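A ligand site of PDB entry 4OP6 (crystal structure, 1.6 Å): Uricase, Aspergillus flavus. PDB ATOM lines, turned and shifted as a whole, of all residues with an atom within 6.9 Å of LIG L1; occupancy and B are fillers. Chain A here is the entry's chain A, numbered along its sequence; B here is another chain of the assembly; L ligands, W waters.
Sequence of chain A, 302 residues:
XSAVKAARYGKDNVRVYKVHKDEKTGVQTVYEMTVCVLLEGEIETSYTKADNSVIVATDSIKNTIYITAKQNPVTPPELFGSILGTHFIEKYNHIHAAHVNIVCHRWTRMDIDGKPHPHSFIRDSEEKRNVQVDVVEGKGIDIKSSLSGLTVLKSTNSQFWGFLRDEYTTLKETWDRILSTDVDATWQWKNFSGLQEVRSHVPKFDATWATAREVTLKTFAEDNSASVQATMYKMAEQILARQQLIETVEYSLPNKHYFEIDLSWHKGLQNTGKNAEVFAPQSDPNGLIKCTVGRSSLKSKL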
ATOM      1  N   SER A 158       4.226  -8.134   0.315  1.00  0.00           N
ATOM      2  CA  SER A 158       4.504  -9.523   0.624  1.00  0.00           C
ATOM      3  C   SER A 158       5.190 -10.079  -0.616  1.00  0.00           C
ATOM      4  O   SER A 158       4.778  -9.794  -1.742  1.00  0.00           O
ATOM      5  CB  SER A 158       3.217 -10.297   0.922  1.00  0.00           C
ATOM      6  OG  SER A 158       3.486 -11.696   0.975  1.00  0.00           O
ATOM      7  N   GLN A 159       6.242 -10.853  -0.387  1.00  0.00           N
ATOM      8  CA  GLN A 159       7.025 -11.447  -1.448  1.00  0.00           C
ATOM      9  C   GLN A 159       7.229 -12.914  -1.133  1.00  0.00           C
ATOM     10  O   GLN A 159       7.117 -13.351   0.027  1.00  0.00           O
ATOM     11  CB  GLN A 159       8.419 -10.770  -1.518  1.00  0.00           C
ATOM     12  CG  GLN A 159       8.349  -9.245  -1.482  1.00  0.00           C
ATOM     13  CD  GLN A 159       9.688  -8.596  -1.767  1.00  0.00           C
ATOM     14  OE1 GLN A 159      10.730  -9.262  -1.834  1.00  0.00           O
ATOM     15  NE2 GLN A 159       9.664  -7.285  -1.954  1.00  0.00           N
ATOM     16  N   PHE A 160       7.567 -13.682  -2.159  1.00  0.00           N
ATOM     17  CA  PHE A 160       7.995 -15.059  -1.943  1.00  0.00           C
ATOM     18  C   PHE A 160       8.845 -15.529  -3.108  1.00  0.00           C
ATOM     19  O   PHE A 160       8.331 -15.883  -4.166  1.00  0.00           O
ATOM     20  CB  PHE A 160       6.800 -16.015  -1.658  1.00  0.00           C
ATOM     21  CG  PHE A 160       7.233 -17.350  -1.138  1.00  0.00           C
ATOM     22  CD1 PHE A 160       7.916 -17.455   0.079  1.00  0.00           C
ATOM     23  CD2 PHE A 160       7.009 -18.511  -1.886  1.00  0.00           C
ATOM     24  CE1 PHE A 160       8.357 -18.695   0.551  1.00  0.00           C
ATOM     25  CE2 PHE A 160       7.442 -19.748  -1.419  1.00  0.00           C
ATOM     26  CZ  PHE A 160       8.140 -19.833  -0.214  1.00  0.00           C
ATOM     27  N   PHE A 163      12.874 -19.867  -3.092  1.00  0.00           N
ATOM     28  CA  PHE A 163      12.597 -21.189  -2.564  1.00  0.00           C
ATOM     29  C   PHE A 163      13.177 -22.308  -3.435  1.00  0.00           C
ATOM     30  O   PHE A 163      13.573 -22.060  -4.580  1.00  0.00           O
ATOM     31  CB  PHE A 163      11.071 -21.413  -2.369  1.00  0.00           C
ATOM     32  CG  PHE A 163      10.256 -21.041  -3.570  1.00  0.00           C
ATOM     33  CD1 PHE A 163       9.775 -19.751  -3.719  1.00  0.00           C
ATOM     34  CD2 PHE A 163       9.959 -22.007  -4.553  1.00  0.00           C
ATOM     35  CE1 PHE A 163       9.012 -19.385  -4.826  1.00  0.00           C
ATOM     36  CE2 PHE A 163       9.192 -21.641  -5.652  1.00  0.00           C
ATOM     37  CZ  PHE A 163       8.737 -20.339  -5.795  1.00  0.00           C
ATOM     38  N   LEU A 171       5.471 -23.332  -9.029  1.00  0.00           N
ATOM     39  CA  LEU A 171       5.207 -21.992  -8.500  1.00  0.00           C
ATOM     40  C   LEU A 171       6.216 -20.960  -9.018  1.00  0.00           C
ATOM     41  O   LEU A 171       7.433 -21.187  -8.942  1.00  0.00           O
ATOM     42  CB  LEU A 171       5.266 -22.046  -6.965  1.00  0.00           C
ATOM     43  CG  LEU A 171       4.937 -20.734  -6.205  1.00  0.00           C
ATOM     44  CD1 LEU A 171       3.468 -20.343  -6.408  1.00  0.00           C
ATOM     45  CD2 LEU A 171       5.233 -20.903  -4.729  1.00  0.00           C
ATOM     46  N   ARG A 177       2.716  -9.877  -3.812  1.00  0.00           N
ATOM     47  CA  ARG A 177       1.514 -10.733  -3.750  1.00  0.00           C
ATOM     48  C   ARG A 177       0.632 -10.280  -2.607  1.00  0.00           C
ATOM     49  O   ARG A 177       1.032  -9.483  -1.747  1.00  0.00           O
ATOM     50  CB  ARG A 177       1.902 -12.200  -3.554  1.00  0.00           C
ATOM     51  CG  ARG A 177       2.553 -12.447  -2.201  1.00  0.00           C
ATOM     52  CD  ARG A 177       2.933 -13.915  -2.033  1.00  0.00           C
ATOM     53  NE  ARG A 177       3.377 -14.143  -0.656  1.00  0.00           N
ATOM     54  CZ  ARG A 177       3.617 -15.336  -0.108  1.00  0.00           C
ATOM     55  NH1 ARG A 177       3.486 -16.471  -0.807  1.00  0.00           N
ATOM     56  NH2 ARG A 177       4.021 -15.376   1.161  1.00  0.00           N
ATOM     57  N   LEU A 179      -1.245 -11.201   0.850  1.00  0.00           N
ATOM     58  CA  LEU A 179      -1.051 -12.117   1.972  1.00  0.00           C
ATOM     59  C   LEU A 179      -2.266 -11.976   2.891  1.00  0.00           C
ATOM     60  O   LEU A 179      -2.579 -10.891   3.384  1.00  0.00           O
ATOM     61  CB  LEU A 179       0.257 -11.787   2.716  1.00  0.00           C
ATOM     62  CG  LEU A 179       0.559 -12.643   3.946  1.00  0.00           C
ATOM     63  CD1 LEU A 179       0.607 -14.117   3.554  1.00  0.00           C
ATOM     64  CD2 LEU A 179       1.888 -12.204   4.569  1.00  0.00           C
ATOM     65  N   SER A 225       7.177  -8.545   3.910  1.00  0.00           N
ATOM     66  CA  SER A 225       7.284  -9.933   4.276  1.00  0.00           C
ATOM     67  C   SER A 225       8.034 -10.780   3.235  1.00  0.00           C
ATOM     68  O   SER A 225       7.689 -10.776   2.049  1.00  0.00           O
ATOM     69  CB  SER A 225       5.867 -10.481   4.494  1.00  0.00           C
ATOM     70  OG  SER A 225       5.942 -11.875   4.744  1.00  0.00           O
ATOM     71  N   ALA A 226       9.039 -11.502   3.700  1.00  0.00           N
ATOM     72  CA  ALA A 226       9.812 -12.370   2.851  1.00  0.00           C
ATOM     73  C   ALA A 226       9.152 -13.746   2.725  1.00  0.00           C
ATOM     74  O   ALA A 226       9.476 -14.532   1.831  1.00  0.00           O
ATOM     75  CB  ALA A 226      11.226 -12.516   3.416  1.00  0.00           C
ATOM     76  N   SER A 227       8.228 -14.041   3.659  1.00  0.00           N
ATOM     77  CA  SER A 227       7.505 -15.318   3.725  1.00  0.00           C
ATOM     78  C   SER A 227       6.630 -15.233   4.967  1.00  0.00           C
ATOM     79  O   SER A 227       6.848 -14.387   5.832  1.00  0.00           O
ATOM     80  CB  SER A 227       8.419 -16.552   3.858  1.00  0.00           C
ATOM     81  OG  SER A 227       9.177 -16.521   5.086  1.00  0.00           O
ATOM     82  N   VAL A 228       5.663 -16.153   5.067  1.00  0.00           N
ATOM     83  CA  VAL A 228       4.875 -16.224   6.283  1.00  0.00           C
ATOM     84  C   VAL A 228       5.789 -16.584   7.453  1.00  0.00           C
ATOM     85  O   VAL A 228       5.652 -16.037   8.545  1.00  0.00           O
ATOM     86  CB  VAL A 228       3.745 -17.268   6.116  1.00  0.00           C
ATOM     87  CG1 VAL A 228       3.021 -17.478   7.434  1.00  0.00           C
ATOM     88  CG2 VAL A 228       2.786 -16.750   5.047  1.00  0.00           C
ATOM     89  N   GLN A 229       6.703 -17.534   7.213  1.00  0.00           N
ATOM     90  CA  GLN A 229       7.694 -18.008   8.198  1.00  0.00           C
ATOM     91  C   GLN A 229       8.428 -16.816   8.811  1.00  0.00           C
ATOM     92  O   GLN A 229       8.512 -16.676  10.053  1.00  0.00           O
ATOM     93  CB  GLN A 229       8.697 -18.936   7.504  1.00  0.00           C
ATOM     94  CG  GLN A 229       8.161 -20.329   7.183  1.00  0.00           C
ATOM     95  CD  GLN A 229       7.474 -20.435   5.829  1.00  0.00           C
ATOM     96  OE1 GLN A 229       6.970 -19.455   5.275  1.00  0.00           O
ATOM     97  NE2 GLN A 229       7.435 -21.659   5.303  1.00  0.00           N
ATOM     98  N   ALA A 230       8.983 -15.940   7.966  1.00  0.00           N
ATOM     99  CA  ALA A 230       9.822 -14.870   8.484  1.00  0.00           C
ATOM    100  C   ALA A 230       9.023 -13.817   9.258  1.00  0.00           C
ATOM    101  O   ALA A 230       9.475 -13.326  10.308  1.00  0.00           O
ATOM    102  CB  ALA A 230      10.597 -14.236   7.335  1.00  0.00           C
ATOM    103  N   ASN A 255      -2.075 -19.811   4.915  1.00  0.00           N
ATOM    104  CA  ASN A 255      -1.815 -18.863   3.850  1.00  0.00           C
ATOM    105  C   ASN A 255      -3.018 -18.992   2.912  1.00  0.00           C
ATOM    106  O   ASN A 255      -3.124 -19.975   2.217  1.00  0.00           O
ATOM    107  CB  ASN A 255      -0.477 -19.228   3.184  1.00  0.00           C
ATOM    108  CG  ASN A 255      -0.023 -18.160   2.192  1.00  0.00           C
ATOM    109  OD1 ASN A 255      -0.705 -17.172   1.976  1.00  0.00           O
ATOM    110  ND2 ASN A 255       1.132 -18.395   1.549  1.00  0.00           N
ATOM    111  N   HIS A 257      -4.850 -18.261  -0.167  1.00  0.00           N
ATOM    112  CA  HIS A 257      -4.364 -17.787  -1.465  1.00  0.00           C
ATOM    113  C   HIS A 257      -5.369 -16.997  -2.247  1.00  0.00           C
ATOM    114  O   HIS A 257      -6.547 -17.337  -2.314  1.00  0.00           O
ATOM    115  CB  HIS A 257      -3.893 -18.969  -2.303  1.00  0.00           C
ATOM    116  CG  HIS A 257      -2.905 -19.853  -1.599  1.00  0.00           C
ATOM    117  ND1 HIS A 257      -1.705 -19.392  -1.177  1.00  0.00           N
ATOM    118  CD2 HIS A 257      -2.983 -21.183  -1.217  1.00  0.00           C
ATOM    119  CE1 HIS A 257      -1.023 -20.407  -0.594  1.00  0.00           C
ATOM    120  NE2 HIS A 257      -1.823 -21.496  -0.600  1.00  0.00           N
ATOM    121  N   GLY A 287      -1.906 -23.042   2.348  1.00  0.00           N
ATOM    122  CA  GLY A 287      -0.683 -23.264   3.131  1.00  0.00           C
ATOM    123  C   GLY A 287      -0.995 -23.257   4.621  1.00  0.00           C
ATOM    124  O   GLY A 287      -1.965 -22.653   5.076  1.00  0.00           O
ATOM    125  N   ILE A 289       1.363 -22.878   8.187  1.00  0.00           N
ATOM    126  CA  ILE A 289       2.726 -22.640   8.675  1.00  0.00           C
ATOM    127  C   ILE A 289       2.678 -22.495  10.178  1.00  0.00           C
ATOM    128  O   ILE A 289       1.899 -21.704  10.696  1.00  0.00           O
ATOM    129  CB  ILE A 289       3.284 -21.309   8.101  1.00  0.00           C
ATOM    130  CG1 ILE A 289       2.965 -21.148   6.597  1.00  0.00           C
ATOM    131  CG2 ILE A 289       4.792 -21.222   8.350  1.00  0.00           C
ATOM    132  CD1 ILE A 289       3.507 -22.209   5.706  1.00  0.00           C
ATOM    133  N   TYR B   9       5.484 -27.060   8.547  1.00  0.00           N
ATOM    134  CA  TYR B   9       4.758 -26.236   7.577  1.00  0.00           C
ATOM    135  C   TYR B   9       4.380 -27.156   6.413  1.00  0.00           C
ATOM    136  O   TYR B   9       4.990 -28.218   6.185  1.00  0.00           O
ATOM    137  CB  TYR B   9       5.589 -25.018   7.112  1.00  0.00           C
ATOM    138  CG  TYR B   9       6.516 -25.419   6.013  1.00  0.00           C
ATOM    139  CD1 TYR B   9       7.616 -26.227   6.283  1.00  0.00           C
ATOM    140  CD2 TYR B   9       6.242 -25.093   4.692  1.00  0.00           C
ATOM    141  CE1 TYR B   9       8.441 -26.685   5.270  1.00  0.00           C
ATOM    142  CE2 TYR B   9       7.054 -25.534   3.672  1.00  0.00           C
ATOM    143  CZ  TYR B   9       8.145 -26.347   3.972  1.00  0.00           C
ATOM    144  OH  TYR B   9       8.949 -26.799   2.957  1.00  0.00           O
ATOM    145  N   GLY B  10       3.358 -26.764   5.665  1.00  0.00           N
ATOM    146  CA  GLY B  10       2.973 -27.572   4.528  1.00  0.00           C
ATOM    147  C   GLY B  10       1.646 -27.136   3.943  1.00  0.00           C
ATOM    148  O   GLY B  10       1.316 -25.974   3.967  1.00  0.00           O
ATOM    149  N   LYS B  11       0.892 -28.082   3.394  1.00  0.00           N
ATOM    150  CA  LYS B  11      -0.349 -27.745   2.679  1.00  0.00           C
ATOM    151  C   LYS B  11      -1.479 -28.489   3.331  1.00  0.00           C
ATOM    152  O   LYS B  11      -1.362 -29.693   3.585  1.00  0.00           O
ATOM    153  CB  LYS B  11      -0.272 -28.137   1.201  1.00  0.00           C
ATOM    154  CG  LYS B  11      -1.247 -27.362   0.318  1.00  0.00           C
ATOM    155  CD  LYS B  11      -0.778 -25.911   0.220  1.00  0.00           C
ATOM    156  CE  LYS B  11      -1.001 -25.253  -1.117  1.00  0.00           C
ATOM    157  NZ  LYS B  11      -0.359 -23.896  -1.158  1.00  0.00           N
ATOM    158  N   ASN B  52      14.808 -18.600   2.191  1.00  0.00           N
ATOM    159  CA  ASN B  52      13.832 -19.495   1.550  1.00  0.00           C
ATOM    160  C   ASN B  52      14.431 -20.717   0.862  1.00  0.00           C
ATOM    161  O   ASN B  52      13.695 -21.583   0.401  1.00  0.00           O
ATOM    162  CB  ASN B  52      12.881 -18.708   0.636  1.00  0.00           C
ATOM    163  CG  ASN B  52      11.993 -17.743   1.394  1.00  0.00           C
ATOM    164  OD1 ASN B  52      11.759 -17.933   2.600  1.00  0.00           O
ATOM    165  ND2 ASN B  52      11.493 -16.715   0.726  1.00  0.00           N
ATOM    166  N   ILE B  55      13.130 -24.021   1.882  1.00  0.00           N
ATOM    167  CA  ILE B  55      11.689 -24.278   1.772  1.00  0.00           C
ATOM    168  C   ILE B  55      11.305 -25.007   0.486  1.00  0.00           C
ATOM    169  O   ILE B  55      11.517 -24.485  -0.615  1.00  0.00           O
ATOM    170  CB  ILE B  55      10.862 -22.976   1.830  1.00  0.00           C
ATOM    171  CG1 ILE B  55      11.088 -22.236   3.158  1.00  0.00           C
ATOM    172  CG2 ILE B  55       9.361 -23.310   1.664  1.00  0.00           C
ATOM    173  CD1 ILE B  55      10.408 -20.870   3.184  1.00  0.00           C
ATOM    174  N   VAL B  56      10.764 -26.210   0.652  1.00  0.00           N
ATOM    175  CA  VAL B  56      10.020 -26.900  -0.387  1.00  0.00           C
ATOM    176  C   VAL B  56       8.670 -26.179  -0.371  1.00  0.00           C
ATOM    177  O   VAL B  56       7.958 -26.261   0.631  1.00  0.00           O
ATOM    178  CB  VAL B  56       9.879 -28.406  -0.045  1.00  0.00           C
ATOM    179  CG1 VAL B  56       8.982 -29.133  -1.065  1.00  0.00           C
ATOM    180  CG2 VAL B  56      11.262 -29.050  -0.022  1.00  0.00           C
ATOM    181  N   ALA B  57       8.333 -25.456  -1.455  1.00  0.00           N
ATOM    182  CA  ALA B  57       7.113 -24.615  -1.466  1.00  0.00           C
ATOM    183  C   ALA B  57       5.888 -25.467  -1.181  1.00  0.00           C
ATOM    184  O   ALA B  57       5.803 -26.606  -1.612  1.00  0.00           O
ATOM    185  CB  ALA B  57       6.954 -23.882  -2.792  1.00  0.00           C
ATOM    186  N   THR B  58       4.925 -24.890  -0.450  1.00  0.00           N
ATOM    187  CA  THR B  58       3.734 -25.665  -0.126  1.00  0.00           C
ATOM    188  C   THR B  58       2.986 -25.993  -1.415  1.00  0.00           C
ATOM    189  O   THR B  58       2.371 -27.060  -1.503  1.00  0.00           O
ATOM    190  CB  THR B  58       2.808 -24.949   0.864  1.00  0.00           C
ATOM    191  OG1 THR B  58       2.237 -23.804   0.231  1.00  0.00           O
ATOM    192  CG2 THR B  58       3.585 -24.500   2.109  1.00  0.00           C
ATOM    193  N   ASP B  59       3.050 -25.105  -2.408  1.00  0.00           N
ATOM    194  CA  ASP B  59       2.511 -25.417  -3.741  1.00  0.00           C
ATOM    195  C   ASP B  59       3.122 -26.686  -4.340  1.00  0.00           C
ATOM    196  O   ASP B  59       2.432 -27.494  -4.959  1.00  0.00           O
ATOM    197  CB  ASP B  59       2.704 -24.255  -4.692  1.00  0.00           C
ATOM    198  CG  ASP B  59       1.930 -24.429  -5.975  1.00  0.00           C
ATOM    199  OD1 ASP B  59       0.689 -24.244  -5.938  1.00  0.00           O
ATOM    200  OD2 ASP B  59       2.570 -24.744  -7.014  1.00  0.00           O
ATOM    201  N   SER B  60       4.437 -26.876  -4.175  1.00  0.00           N
ATOM    202  CA  SER B  60       5.096 -28.124  -4.612  1.00  0.00           C
ATOM    203  C   SER B  60       4.640 -29.349  -3.846  1.00  0.00           C
ATOM    204  O   SER B  60       4.542 -30.432  -4.401  1.00  0.00           O
ATOM    205  CB  SER B  60       6.631 -27.981  -4.532  1.00  0.00           C
ATOM    206  OG  SER B  60       7.004 -26.792  -5.187  1.00  0.00           O
HETATM  207  N1  LIG L   1       5.635 -19.700   2.662  1.00  0.00           N
HETATM  208  C1  LIG L   1       5.027 -18.663   2.033  1.00  0.00           C
HETATM  209  O1  LIG L   1       5.010 -17.580   2.633  1.00  0.00           O
HETATM  210  N2  LIG L   1       4.413 -18.757   0.811  1.00  0.00           N
HETATM  211  C2  LIG L   1       4.469 -19.927   0.170  1.00  0.00           C
HETATM  212  C3  LIG L   1       5.122 -21.093   0.796  1.00  0.00           C
HETATM  213  C4  LIG L   1       5.735 -20.916   2.118  1.00  0.00           C
HETATM  214  O2  LIG L   1       6.259 -21.884   2.686  1.00  0.00           O
HETATM  215  N3  LIG L   1       5.028 -22.130  -0.039  1.00  0.00           N
HETATM  216  N4  LIG L   1       4.335 -21.706  -1.158  1.00  0.00           N
HETATM  217  N5  LIG L   1       4.007 -20.371  -1.015  1.00  0.00           N
HETATM  218  O1  LG2 L   2       2.043 -21.407   2.320  1.00  0.00           O
HETATM  219  O2  LG2 L   2       1.564 -21.476   1.364  1.00  0.00           O
HETATM  220  O   HOH W   1       2.244 -19.020  -2.614  1.00  0.00           O
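Water W1 lies within hydrogen-bond range of N5 of LIG L1 and NH1 of Arg 177.
N of Gln 229 lies close to OG of Ser 227. The backbone carbonyl oxygen (O) of Ser 227 lies within hydrogen-bond range of the side-chain hydroxyl (OG) of Ser 225 (2.9 Å). The backbone NH (N) of Ala 230 is in hydrogen-bond range of the side-chain hydroxyl (OG) of Ser 227 (2.9 Å). N of Asn 255 is in hydrogen-bond range of O of Gly 287, 2.8 Å away. The backbone NH (N) of Arg 177 lies within hydrogen-bond range of the backbone carbonyl oxygen (O) of Ser 158 (2.9 Å). The side-chain hydroxyl (OG1) of Thr 58 of chain B lies within hydrogen-bond range of the side-chain amino group (NZ) of Lys 11 of chain B (2.9 Å). The side-chain hydroxyl (OH) of Tyr 9 of chain B lies within hydrogen-bond range of the backbone carbonyl oxygen (O) of Val 56 of chain B (2.6 Å). O of Asn 255 sits at hydrogen-bond distance from NE2 of His 257.
ND2 of Asn 255 sits close to N2 of LIG L1 (3.4 Å). N3 of LIG L1 is in hydrogen-bond range of N of Thr 58 of chain B (2.8 Å). An oxygen (O2) of LIG L1 sits at hydrogen-bond distance from the side-chain amide nitrogen (NE2) of Gln 229 (2.9 Å). NH2 of Arg 177 lies within hydrogen-bond range of O1 of LIG L1. The side-chain hydroxyl of Thr 58 of chain B is in hydrogen-bond range of an oxygen (O2) of LG2 L2. An oxygen (O1) of LIG L1 is in hydrogen-bond range of the backbone NH of Val 228. The side-chain amide nitrogen (ND2) of Asn 255 sits at hydrogen-bond distance from an oxygen (O2) of LG2 L2 (3.1 Å). OG1 of Thr 58 of chain B sits at hydrogen-bond distance from N3 of LIG L1 (3.3 Å).
Merely in contact with LIG L1: Phe 160 (3.4 Å), Leu 171 (3.8 Å), Ser 227 (3.5 Å), Tyr 9 of chain B (3.8 Å), Ile 55 of chain B (3.6 Å), Ala 57 of chain B (3.5 Å) and Asp 59 of chain B (3.8 Å). Hydrophobic or aromatic side chains that line LIG L1: Phe 160, Leu 171, Val 228, Tyr 9 of chain B, Ile 55 of chain B and Ala 57 of chain B. 12 residues have an atom within 4 Å of LIG L1: Phe 160, Leu 171, Arg 177, Ser 227, Val 228, Gln 229, Asn 255, Tyr 9 of chain B, Ile 55 of chain B, Ala 57 of chain B, Thr 58 of chain B and Asp 59 of chain B. The nearest printed residue that does not touch LIG L1 is Ile 289 (4.1 Å).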
